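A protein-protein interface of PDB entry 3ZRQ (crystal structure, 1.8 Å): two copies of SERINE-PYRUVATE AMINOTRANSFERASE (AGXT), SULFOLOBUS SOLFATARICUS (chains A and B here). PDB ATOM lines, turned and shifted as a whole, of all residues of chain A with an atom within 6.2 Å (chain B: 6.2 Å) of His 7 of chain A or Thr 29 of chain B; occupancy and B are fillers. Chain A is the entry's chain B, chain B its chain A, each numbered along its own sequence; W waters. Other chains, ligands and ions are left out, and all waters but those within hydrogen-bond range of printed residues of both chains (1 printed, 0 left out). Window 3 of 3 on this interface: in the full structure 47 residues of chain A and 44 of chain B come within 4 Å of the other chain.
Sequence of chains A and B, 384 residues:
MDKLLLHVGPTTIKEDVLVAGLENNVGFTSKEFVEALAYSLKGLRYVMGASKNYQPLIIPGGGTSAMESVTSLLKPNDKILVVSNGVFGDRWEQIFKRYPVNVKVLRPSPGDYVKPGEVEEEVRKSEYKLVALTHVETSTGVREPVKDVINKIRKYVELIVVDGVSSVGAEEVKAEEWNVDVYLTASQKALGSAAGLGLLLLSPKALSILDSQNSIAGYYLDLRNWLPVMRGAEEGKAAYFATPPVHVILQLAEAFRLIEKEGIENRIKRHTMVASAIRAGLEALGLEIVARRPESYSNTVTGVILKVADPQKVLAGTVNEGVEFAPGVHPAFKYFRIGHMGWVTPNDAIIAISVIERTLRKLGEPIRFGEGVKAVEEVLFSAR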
ATOM      1  N   LEU A   4     -20.849 -30.819   3.998  1.00  0.00           N
ATOM      2  CA  LEU A   4     -20.856 -29.377   3.719  1.00  0.00           C
ATOM      3  C   LEU A   4     -21.958 -28.989   2.733  1.00  0.00           C
ATOM      4  O   LEU A   4     -22.138 -29.656   1.714  1.00  0.00           O
ATOM      5  CB  LEU A   4     -19.508 -28.936   3.134  1.00  0.00           C
ATOM      6  CG  LEU A   4     -18.509 -28.259   4.065  1.00  0.00           C
ATOM      7  CD1 LEU A   4     -17.370 -27.695   3.225  1.00  0.00           C
ATOM      8  CD2 LEU A   4     -19.176 -27.171   4.932  1.00  0.00           C
ATOM      9  N   LEU A   5     -22.677 -27.903   3.028  1.00  0.00           N
ATOM     10  CA  LEU A   5     -23.605 -27.316   2.049  1.00  0.00           C
ATOM     11  C   LEU A   5     -22.952 -26.103   1.369  1.00  0.00           C
ATOM     12  O   LEU A   5     -23.006 -24.978   1.889  1.00  0.00           O
ATOM     13  CB  LEU A   5     -24.984 -26.972   2.664  1.00  0.00           C
ATOM     14  CG  LEU A   5     -26.165 -26.558   1.756  1.00  0.00           C
ATOM     15  CD1 LEU A   5     -26.611 -27.654   0.784  1.00  0.00           C
ATOM     16  CD2 LEU A   5     -27.370 -26.113   2.588  1.00  0.00           C
ATOM     17  N   LEU A   6     -22.311 -26.367   0.226  1.00  0.00           N
ATOM     18  CA  LEU A   6     -21.749 -25.328  -0.641  1.00  0.00           C
ATOM     19  C   LEU A   6     -22.639 -25.157  -1.882  1.00  0.00           C
ATOM     20  O   LEU A   6     -22.192 -25.320  -3.039  1.00  0.00           O
ATOM     21  CB  LEU A   6     -20.284 -25.649  -0.992  1.00  0.00           C
ATOM     22  CG  LEU A   6     -19.240 -25.538   0.145  1.00  0.00           C
ATOM     23  CD1 LEU A   6     -17.817 -25.792  -0.398  1.00  0.00           C
ATOM     24  CD2 LEU A   6     -19.282 -24.185   0.888  1.00  0.00           C
ATOM     25  N   HIS A   7     -23.908 -24.848  -1.588  1.00  0.00           N
ATOM     26  CA  HIS A   7     -24.998 -24.648  -2.552  1.00  0.00           C
ATOM     27  C   HIS A   7     -25.227 -23.125  -2.682  1.00  0.00           C
ATOM     28  O   HIS A   7     -24.497 -22.298  -2.086  1.00  0.00           O
ATOM     29  CB  HIS A   7     -26.281 -25.359  -2.037  1.00  0.00           C
ATOM     30  CG  HIS A   7     -27.243 -25.799  -3.111  1.00  0.00           C
ATOM     31  ND1 HIS A   7     -28.083 -24.927  -3.777  1.00  0.00           N
ATOM     32  CD2 HIS A   7     -27.530 -27.032  -3.598  1.00  0.00           C
ATOM     33  CE1 HIS A   7     -28.820 -25.596  -4.645  1.00  0.00           C
ATOM     34  NE2 HIS A   7     -28.511 -26.877  -4.552  1.00  0.00           N
ATOM     35  N   VAL A   8     -26.260 -22.760  -3.434  1.00  0.00           N
ATOM     36  CA  VAL A   8     -26.562 -21.359  -3.711  1.00  0.00           C
ATOM     37  C   VAL A   8     -27.502 -20.677  -2.688  1.00  0.00           C
ATOM     38  O   VAL A   8     -27.894 -19.535  -2.890  1.00  0.00           O
ATOM     39  CB  VAL A   8     -27.057 -21.184  -5.170  1.00  0.00           C
ATOM     40  CG1 VAL A   8     -25.987 -21.684  -6.144  1.00  0.00           C
ATOM     41  CG2 VAL A   8     -28.394 -21.922  -5.409  1.00  0.00           C
ATOM     42  N   GLY A   9     -27.833 -21.374  -1.597  1.00  0.00           N
ATOM     43  CA  GLY A   9     -28.696 -20.828  -0.535  1.00  0.00           C
ATOM     44  C   GLY A   9     -30.004 -21.591  -0.316  1.00  0.00           C
ATOM     45  O   GLY A   9     -30.767 -21.779  -1.261  1.00  0.00           O
ATOM     46  N   PRO A  10     -30.267 -22.060   0.926  1.00  0.00           N
ATOM     47  CA  PRO A  10     -29.353 -22.012   2.072  1.00  0.00           C
ATOM     48  C   PRO A  10     -27.975 -22.607   1.764  1.00  0.00           C
ATOM     49  O   PRO A  10     -27.824 -23.468   0.881  1.00  0.00           O
ATOM     50  CB  PRO A  10     -30.061 -22.856   3.147  1.00  0.00           C
ATOM     51  CG  PRO A  10     -31.505 -22.820   2.794  1.00  0.00           C
ATOM     52  CD  PRO A  10     -31.593 -22.607   1.292  1.00  0.00           C
ATOM     53  N   THR A  11     -26.982 -22.101   2.483  1.00  0.00           N
ATOM     54  CA  THR A  11     -25.652 -22.680   2.525  1.00  0.00           C
ATOM     55  C   THR A  11     -25.561 -23.209   3.969  1.00  0.00           C
ATOM     56  O   THR A  11     -26.599 -23.352   4.630  1.00  0.00           O
ATOM     57  CB  THR A  11     -24.587 -21.612   2.142  1.00  0.00           C
ATOM     58  OG1 THR A  11     -23.284 -22.013   2.583  1.00  0.00           O
ATOM     59  CG2 THR A  11     -24.932 -20.248   2.747  1.00  0.00           C
ATOM     60  N   THR A 300     -19.362 -15.081  -4.722  1.00  0.00           N
ATOM     61  CA  THR A 300     -20.327 -15.967  -4.065  1.00  0.00           C
ATOM     62  C   THR A 300     -20.567 -17.247  -4.821  1.00  0.00           C
ATOM     63  O   THR A 300     -20.899 -18.240  -4.198  1.00  0.00           O
ATOM     64  CB  THR A 300     -21.670 -15.286  -3.808  1.00  0.00           C
ATOM     65  OG1 THR A 300     -22.211 -14.844  -5.056  1.00  0.00           O
ATOM     66  CG2 THR A 300     -21.480 -14.097  -2.888  1.00  0.00           C
ATOM     67  N   GLU A 324     -22.202 -30.888  -0.713  1.00  0.00           N
ATOM     68  CA  GLU A 324     -23.278 -30.657  -1.683  1.00  0.00           C
ATOM     69  C   GLU A 324     -23.018 -29.310  -2.385  1.00  0.00           C
ATOM     70  O   GLU A 324     -23.032 -28.260  -1.737  1.00  0.00           O
ATOM     71  CB  GLU A 324     -24.654 -30.684  -0.993  1.00  0.00           C
ATOM     72  CG  GLU A 324     -25.866 -30.818  -1.935  1.00  0.00           C
ATOM     73  CD  GLU A 324     -27.216 -30.633  -1.226  1.00  0.00           C
ATOM     74  OE1 GLU A 324     -27.329 -30.955  -0.022  1.00  0.00           O
ATOM     75  OE2 GLU A 324     -28.175 -30.160  -1.878  1.00  0.00           O
ATOM     76  N   PHE A 325     -22.724 -29.380  -3.691  1.00  0.00           N
ATOM     77  CA  PHE A 325     -22.585 -28.229  -4.612  1.00  0.00           C
ATOM     78  C   PHE A 325     -23.938 -28.000  -5.324  1.00  0.00           C
ATOM     79  O   PHE A 325     -24.939 -28.586  -4.936  1.00  0.00           O
ATOM     80  CB  PHE A 325     -21.518 -28.548  -5.667  1.00  0.00           C
ATOM     81  CG  PHE A 325     -20.089 -28.602  -5.145  1.00  0.00           C
ATOM     82  CD1 PHE A 325     -19.489 -27.482  -4.557  1.00  0.00           C
ATOM     83  CD2 PHE A 325     -19.328 -29.755  -5.306  1.00  0.00           C
ATOM     84  CE1 PHE A 325     -18.161 -27.531  -4.114  1.00  0.00           C
ATOM     85  CE2 PHE A 325     -17.997 -29.809  -4.874  1.00  0.00           C
ATOM     86  CZ  PHE A 325     -17.415 -28.701  -4.273  1.00  0.00           C
ATOM     87  N   ALA A 326     -23.981 -27.173  -6.368  1.00  0.00           N
ATOM     88  CA  ALA A 326     -25.248 -26.933  -7.108  1.00  0.00           C
ATOM     89  C   ALA A 326     -25.173 -27.315  -8.589  1.00  0.00           C
ATOM     90  O   ALA A 326     -24.096 -27.268  -9.183  1.00  0.00           O
ATOM     91  CB  ALA A 326     -25.689 -25.483  -6.960  1.00  0.00           C
ATOM     92  N   PRO A 327     -26.320 -27.688  -9.202  1.00  0.00           N
ATOM     93  CA  PRO A 327     -26.270 -28.026 -10.625  1.00  0.00           C
ATOM     94  C   PRO A 327     -26.097 -26.788 -11.506  1.00  0.00           C
ATOM     95  O   PRO A 327     -26.406 -25.676 -11.082  1.00  0.00           O
ATOM     96  CB  PRO A 327     -27.630 -28.689 -10.881  1.00  0.00           C
ATOM     97  CG  PRO A 327     -28.526 -28.063  -9.892  1.00  0.00           C
ATOM     98  CD  PRO A 327     -27.684 -27.836  -8.656  1.00  0.00           C
ATOM     99  N   ARG A 337     -21.928 -25.760 -10.184  1.00  0.00           N
ATOM    100  CA  ARG A 337     -21.652 -24.510  -9.474  1.00  0.00           C
ATOM    101  C   ARG A 337     -21.140 -24.712  -8.045  1.00  0.00           C
ATOM    102  O   ARG A 337     -21.656 -25.557  -7.302  1.00  0.00           O
ATOM    103  CB  ARG A 337     -22.914 -23.639  -9.414  1.00  0.00           C
ATOM    104  CG  ARG A 337     -23.335 -23.003 -10.731  1.00  0.00           C
ATOM    105  CD  ARG A 337     -24.613 -22.174 -10.551  1.00  0.00           C
ATOM    106  NE  ARG A 337     -25.762 -23.038 -10.305  1.00  0.00           N
ATOM    107  CZ  ARG A 337     -26.950 -22.649  -9.855  1.00  0.00           C
ATOM    108  NH1 ARG A 337     -27.209 -21.369  -9.612  1.00  0.00           N
ATOM    109  NH2 ARG A 337     -27.904 -23.554  -9.672  1.00  0.00           N
ATOM    110  N   ILE A 338     -20.175 -23.890  -7.646  1.00  0.00           N
ATOM    111  CA  ILE A 338     -19.766 -23.779  -6.245  1.00  0.00           C
ATOM    112  C   ILE A 338     -20.364 -22.536  -5.609  1.00  0.00           C
ATOM    113  O   ILE A 338     -20.186 -21.424  -6.111  1.00  0.00           O
ATOM    114  CB  ILE A 338     -18.225 -23.715  -6.083  1.00  0.00           C
ATOM    115  CG1 ILE A 338     -17.556 -24.853  -6.862  1.00  0.00           C
ATOM    116  CG2 ILE A 338     -17.834 -23.661  -4.584  1.00  0.00           C
ATOM    117  CD1 ILE A 338     -16.046 -24.663  -7.073  1.00  0.00           C
ATOM    118  N   GLY A 339     -21.095 -22.734  -4.516  1.00  0.00           N
ATOM    119  CA  GLY A 339     -21.533 -21.637  -3.668  1.00  0.00           C
ATOM    120  C   GLY A 339     -20.525 -21.445  -2.553  1.00  0.00           C
ATOM    121  O   GLY A 339     -20.293 -22.352  -1.748  1.00  0.00           O
ATOM    122  N   HIS A 340     -19.923 -20.261  -2.504  1.00  0.00           N
ATOM    123  CA  HIS A 340     -18.959 -19.918  -1.476  1.00  0.00           C
ATOM    124  C   HIS A 340     -19.358 -18.591  -0.844  1.00  0.00           C
ATOM    125  O   HIS A 340     -18.857 -17.534  -1.227  1.00  0.00           O
ATOM    126  CB  HIS A 340     -17.519 -19.889  -2.042  1.00  0.00           C
ATOM    127  CG  HIS A 340     -17.413 -19.333  -3.438  1.00  0.00           C
ATOM    128  ND1 HIS A 340     -17.384 -17.981  -3.700  1.00  0.00           N
ATOM    129  CD2 HIS A 340     -17.272 -19.945  -4.637  1.00  0.00           C
ATOM    130  CE1 HIS A 340     -17.247 -17.788  -5.001  1.00  0.00           C
ATOM    131  NE2 HIS A 340     -17.187 -18.960  -5.592  1.00  0.00           N
ATOM    132  N   MET A 341     -20.269 -18.660   0.129  1.00  0.00           N
ATOM    133  CA  MET A 341     -20.889 -17.464   0.676  1.00  0.00           C
ATOM    134  C   MET A 341     -21.422 -17.624   2.099  1.00  0.00           C
ATOM    135  O   MET A 341     -21.700 -18.726   2.534  1.00  0.00           O
ATOM    136  CB  MET A 341     -22.019 -16.989  -0.246  1.00  0.00           C
ATOM    137  CG  MET A 341     -23.305 -17.828  -0.126  1.00  0.00           C
ATOM    138  SD  MET A 341     -24.584 -17.341  -1.318  1.00  0.00           S
ATOM    139  CE  MET A 341     -24.115 -18.388  -2.703  1.00  0.00           C
ATOM    140  N   GLY B  27     -30.946 -27.885   2.444  1.00  0.00           N
ATOM    141  CA  GLY B  27     -31.506 -26.926   1.475  1.00  0.00           C
ATOM    142  C   GLY B  27     -32.658 -27.546   0.697  1.00  0.00           C
ATOM    143  O   GLY B  27     -33.066 -28.672   0.992  1.00  0.00           O
ATOM    144  N   PHE B  28     -33.179 -26.841  -0.311  1.00  0.00           N
ATOM    145  CA  PHE B  28     -34.424 -27.274  -1.006  1.00  0.00           C
ATOM    146  C   PHE B  28     -34.311 -28.540  -1.871  1.00  0.00           C
ATOM    147  O   PHE B  28     -35.327 -29.192  -2.174  1.00  0.00           O
ATOM    148  CB  PHE B  28     -35.056 -26.134  -1.817  1.00  0.00           C
ATOM    149  CG  PHE B  28     -34.109 -25.461  -2.775  1.00  0.00           C
ATOM    150  CD1 PHE B  28     -33.346 -24.364  -2.373  1.00  0.00           C
ATOM    151  CD2 PHE B  28     -33.984 -25.916  -4.087  1.00  0.00           C
ATOM    152  CE1 PHE B  28     -32.477 -23.741  -3.257  1.00  0.00           C
ATOM    153  CE2 PHE B  28     -33.121 -25.287  -4.976  1.00  0.00           C
ATOM    154  CZ  PHE B  28     -32.360 -24.211  -4.567  1.00  0.00           C
ATOM    155  N   THR B  29     -33.081 -28.887  -2.251  1.00  0.00           N
ATOM    156  CA  THR B  29     -32.814 -30.130  -2.979  1.00  0.00           C
ATOM    157  C   THR B  29     -32.435 -31.278  -2.048  1.00  0.00           C
ATOM    158  O   THR B  29     -32.468 -32.437  -2.463  1.00  0.00           O
ATOM    159  CB  THR B  29     -31.679 -29.961  -4.020  1.00  0.00           C
ATOM    160  OG1 THR B  29     -30.421 -29.839  -3.345  1.00  0.00           O
ATOM    161  CG2 THR B  29     -31.893 -28.714  -4.865  1.00  0.00           C
ATOM    162  N   SER B  30     -32.076 -30.961  -0.799  1.00  0.00           N
ATOM    163  CA  SER B  30     -31.623 -31.983   0.165  1.00  0.00           C
ATOM    164  C   SER B  30     -32.686 -33.032   0.408  1.00  0.00           C
ATOM    165  O   SER B  30     -33.881 -32.727   0.435  1.00  0.00           O
ATOM    166  CB  SER B  30     -31.172 -31.372   1.502  1.00  0.00           C
ATOM    167  OG  SER B  30     -30.164 -30.385   1.314  1.00  0.00           O
ATOM    168  N   LYS B  31     -32.231 -34.275   0.555  1.00  0.00           N
ATOM    169  CA  LYS B  31     -33.077 -35.423   0.831  1.00  0.00           C
ATOM    170  C   LYS B  31     -33.967 -35.231   2.066  1.00  0.00           C
ATOM    171  O   LYS B  31     -35.126 -35.660   2.073  1.00  0.00           O
ATOM    172  CB  LYS B  31     -32.186 -36.670   1.011  1.00  0.00           C
ATOM    173  CG  LYS B  31     -32.927 -38.009   1.132  1.00  0.00           C
ATOM    174  CD  LYS B  31     -31.959 -39.211   1.146  1.00  0.00           C
ATOM    175  CE  LYS B  31     -31.693 -39.743  -0.267  1.00  0.00           C
ATOM    176  NZ  LYS B  31     -30.613 -40.775  -0.315  1.00  0.00           N
ATOM    177  N   GLU B  32     -33.424 -34.608   3.119  1.00  0.00           N
ATOM    178  CA  GLU B  32     -34.201 -34.366   4.340  1.00  0.00           C
ATOM    179  C   GLU B  32     -35.375 -33.393   4.092  1.00  0.00           C
ATOM    180  O   GLU B  32     -36.446 -33.563   4.651  1.00  0.00           O
ATOM    181  CB  GLU B  32     -33.308 -33.844   5.473  1.00  0.00           C
ATOM    182  CG  GLU B  32     -32.116 -34.739   5.813  1.00  0.00           C
ATOM    183  CD  GLU B  32     -30.832 -34.357   5.067  1.00  0.00           C
ATOM    184  OE1 GLU B  32     -30.887 -33.985   3.868  1.00  0.00           O
ATOM    185  OE2 GLU B  32     -29.754 -34.445   5.692  1.00  0.00           O
ATOM    186  N   PHE B  33     -35.144 -32.383   3.265  1.00  0.00           N
ATOM    187  CA  PHE B  33     -36.212 -31.449   2.917  1.00  0.00           C
ATOM    188  C   PHE B  33     -37.317 -32.101   2.083  1.00  0.00           C
ATOM    189  O   PHE B  33     -38.495 -32.001   2.412  1.00  0.00           O
ATOM    190  CB  PHE B  33     -35.680 -30.214   2.202  1.00  0.00           C
ATOM    191  CG  PHE B  33     -36.783 -29.338   1.698  1.00  0.00           C
ATOM    192  CD1 PHE B  33     -37.544 -28.595   2.601  1.00  0.00           C
ATOM    193  CD2 PHE B  33     -37.144 -29.344   0.358  1.00  0.00           C
ATOM    194  CE1 PHE B  33     -38.600 -27.795   2.172  1.00  0.00           C
ATOM    195  CE2 PHE B  33     -38.222 -28.575  -0.099  1.00  0.00           C
ATOM    196  CZ  PHE B  33     -38.962 -27.793   0.815  1.00  0.00           C
ATOM    197  N   VAL B  34     -36.931 -32.777   1.000  1.00  0.00           N
ATOM    198  CA  VAL B  34     -37.898 -33.452   0.134  1.00  0.00           C
ATOM    199  C   VAL B  34     -38.804 -34.369   0.942  1.00  0.00           C
ATOM    200  O   VAL B  34     -40.030 -34.346   0.758  1.00  0.00           O
ATOM    201  CB  VAL B  34     -37.202 -34.203  -1.042  1.00  0.00           C
ATOM    202  CG1 VAL B  34     -38.188 -35.097  -1.793  1.00  0.00           C
ATOM    203  CG2 VAL B  34     -36.555 -33.184  -1.983  1.00  0.00           C
ATOM    204  N   ALA B 238     -36.739 -33.527  -6.187  1.00  0.00           N
ATOM    205  CA  ALA B 238     -36.634 -32.118  -5.873  1.00  0.00           C
ATOM    206  C   ALA B 238     -36.937 -31.320  -7.133  1.00  0.00           C
ATOM    207  O   ALA B 238     -36.596 -31.737  -8.238  1.00  0.00           O
ATOM    208  CB  ALA B 238     -35.242 -31.792  -5.354  1.00  0.00           C
HETATM  209  O   HOH W   1     -30.111 -27.903  -1.191  1.00  0.00           O
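No position is printed for both chains.
Of the 18 printed residues of chain A, 4 touch a printed residue of chain B. Along chain A the printed residues that touch a printed residue of chain B span positions 5 to 324. Printed residues of chain B that touch a printed residue of chain A: Gly 27, Phe 28, Thr 29 and Ser 30. Hydrophobic or aromatic side chains of chain B that line the printed part of chain A: Phe 28. Along chain B the printed residues that touch a printed residue of chain A span positions 27 to 30. Among the printed residues, 6 pairs touch across the chains.
The backbone NH of Leu 6 of chain A lies within hydrogen-bond range of the backbone carbonyl oxygen of Glu 324 of chain A (2.8 Å). OG1 of Thr 11 of chain A lies within hydrogen-bond range of O of Leu 5 of chain A (3.1 Å). OG of Ser 30 of chain B lies within hydrogen-bond range of N of Gly 27 of chain B (2.9 Å). The backbone NH (N) of Glu 324 of chain A lies within hydrogen-bond range of the backbone carbonyl oxygen (O) of Leu 4 of chain A (2.7 Å).
Leu 4 of chain A touches none of the printed residues of chain B. Printed residues of chain B within 4 Å of Gly 9 of chain A: Phe 28 (3.3 Å). Thr 11 of chain A touches none of the printed residues of chain B. Printed residues of chain B within 4 Å of Glu 324 of chain A: Thr 29 (2.7 Å) and Ser 30 (3.2 Å). Of the printed residues of chain A, Gly 27 of chain B touches Leu 5. Of the printed residues of chain A, Phe 28 of chain B touches His 7 and Gly 9. Thr 29 of chain B touches two residues of chain A. The nearest printed residue of chain B that does not touch His 7 of chain A is Gly 27 of chain B (6.4 Å).
Water W1 lies within hydrogen-bond range of the side-chain hydroxyl of Thr 29 of chain B, the side-chain carboxylate of Glu 324 of chain A and the backbone NH of Phe 28 of chain B.
The side-chain hydroxyl (OG) of Ser 30 of chain B sits at hydrogen-bond distance from the side-chain carboxylate (OE1) of Glu 324 of chain A (3.2 Å). The side-chain carboxylate (OE2) of Glu 324 of chain A lies within hydrogen-bond range of the side-chain hydroxyl (OG1) of Thr 29 of chain B, at 2.7 Å.
Among the printed residues, merely in contact across the chains: Gly 9 of chain A with Phe 28 of chain B (3.3 Å), His 7 of chain A with Thr 29 of chain B (3.7 Å), His 7 of chain A with Phe 28 of chain B (3.8 Å) and Leu 5 of chain A with Gly 27 of chain B (3.99 Å).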
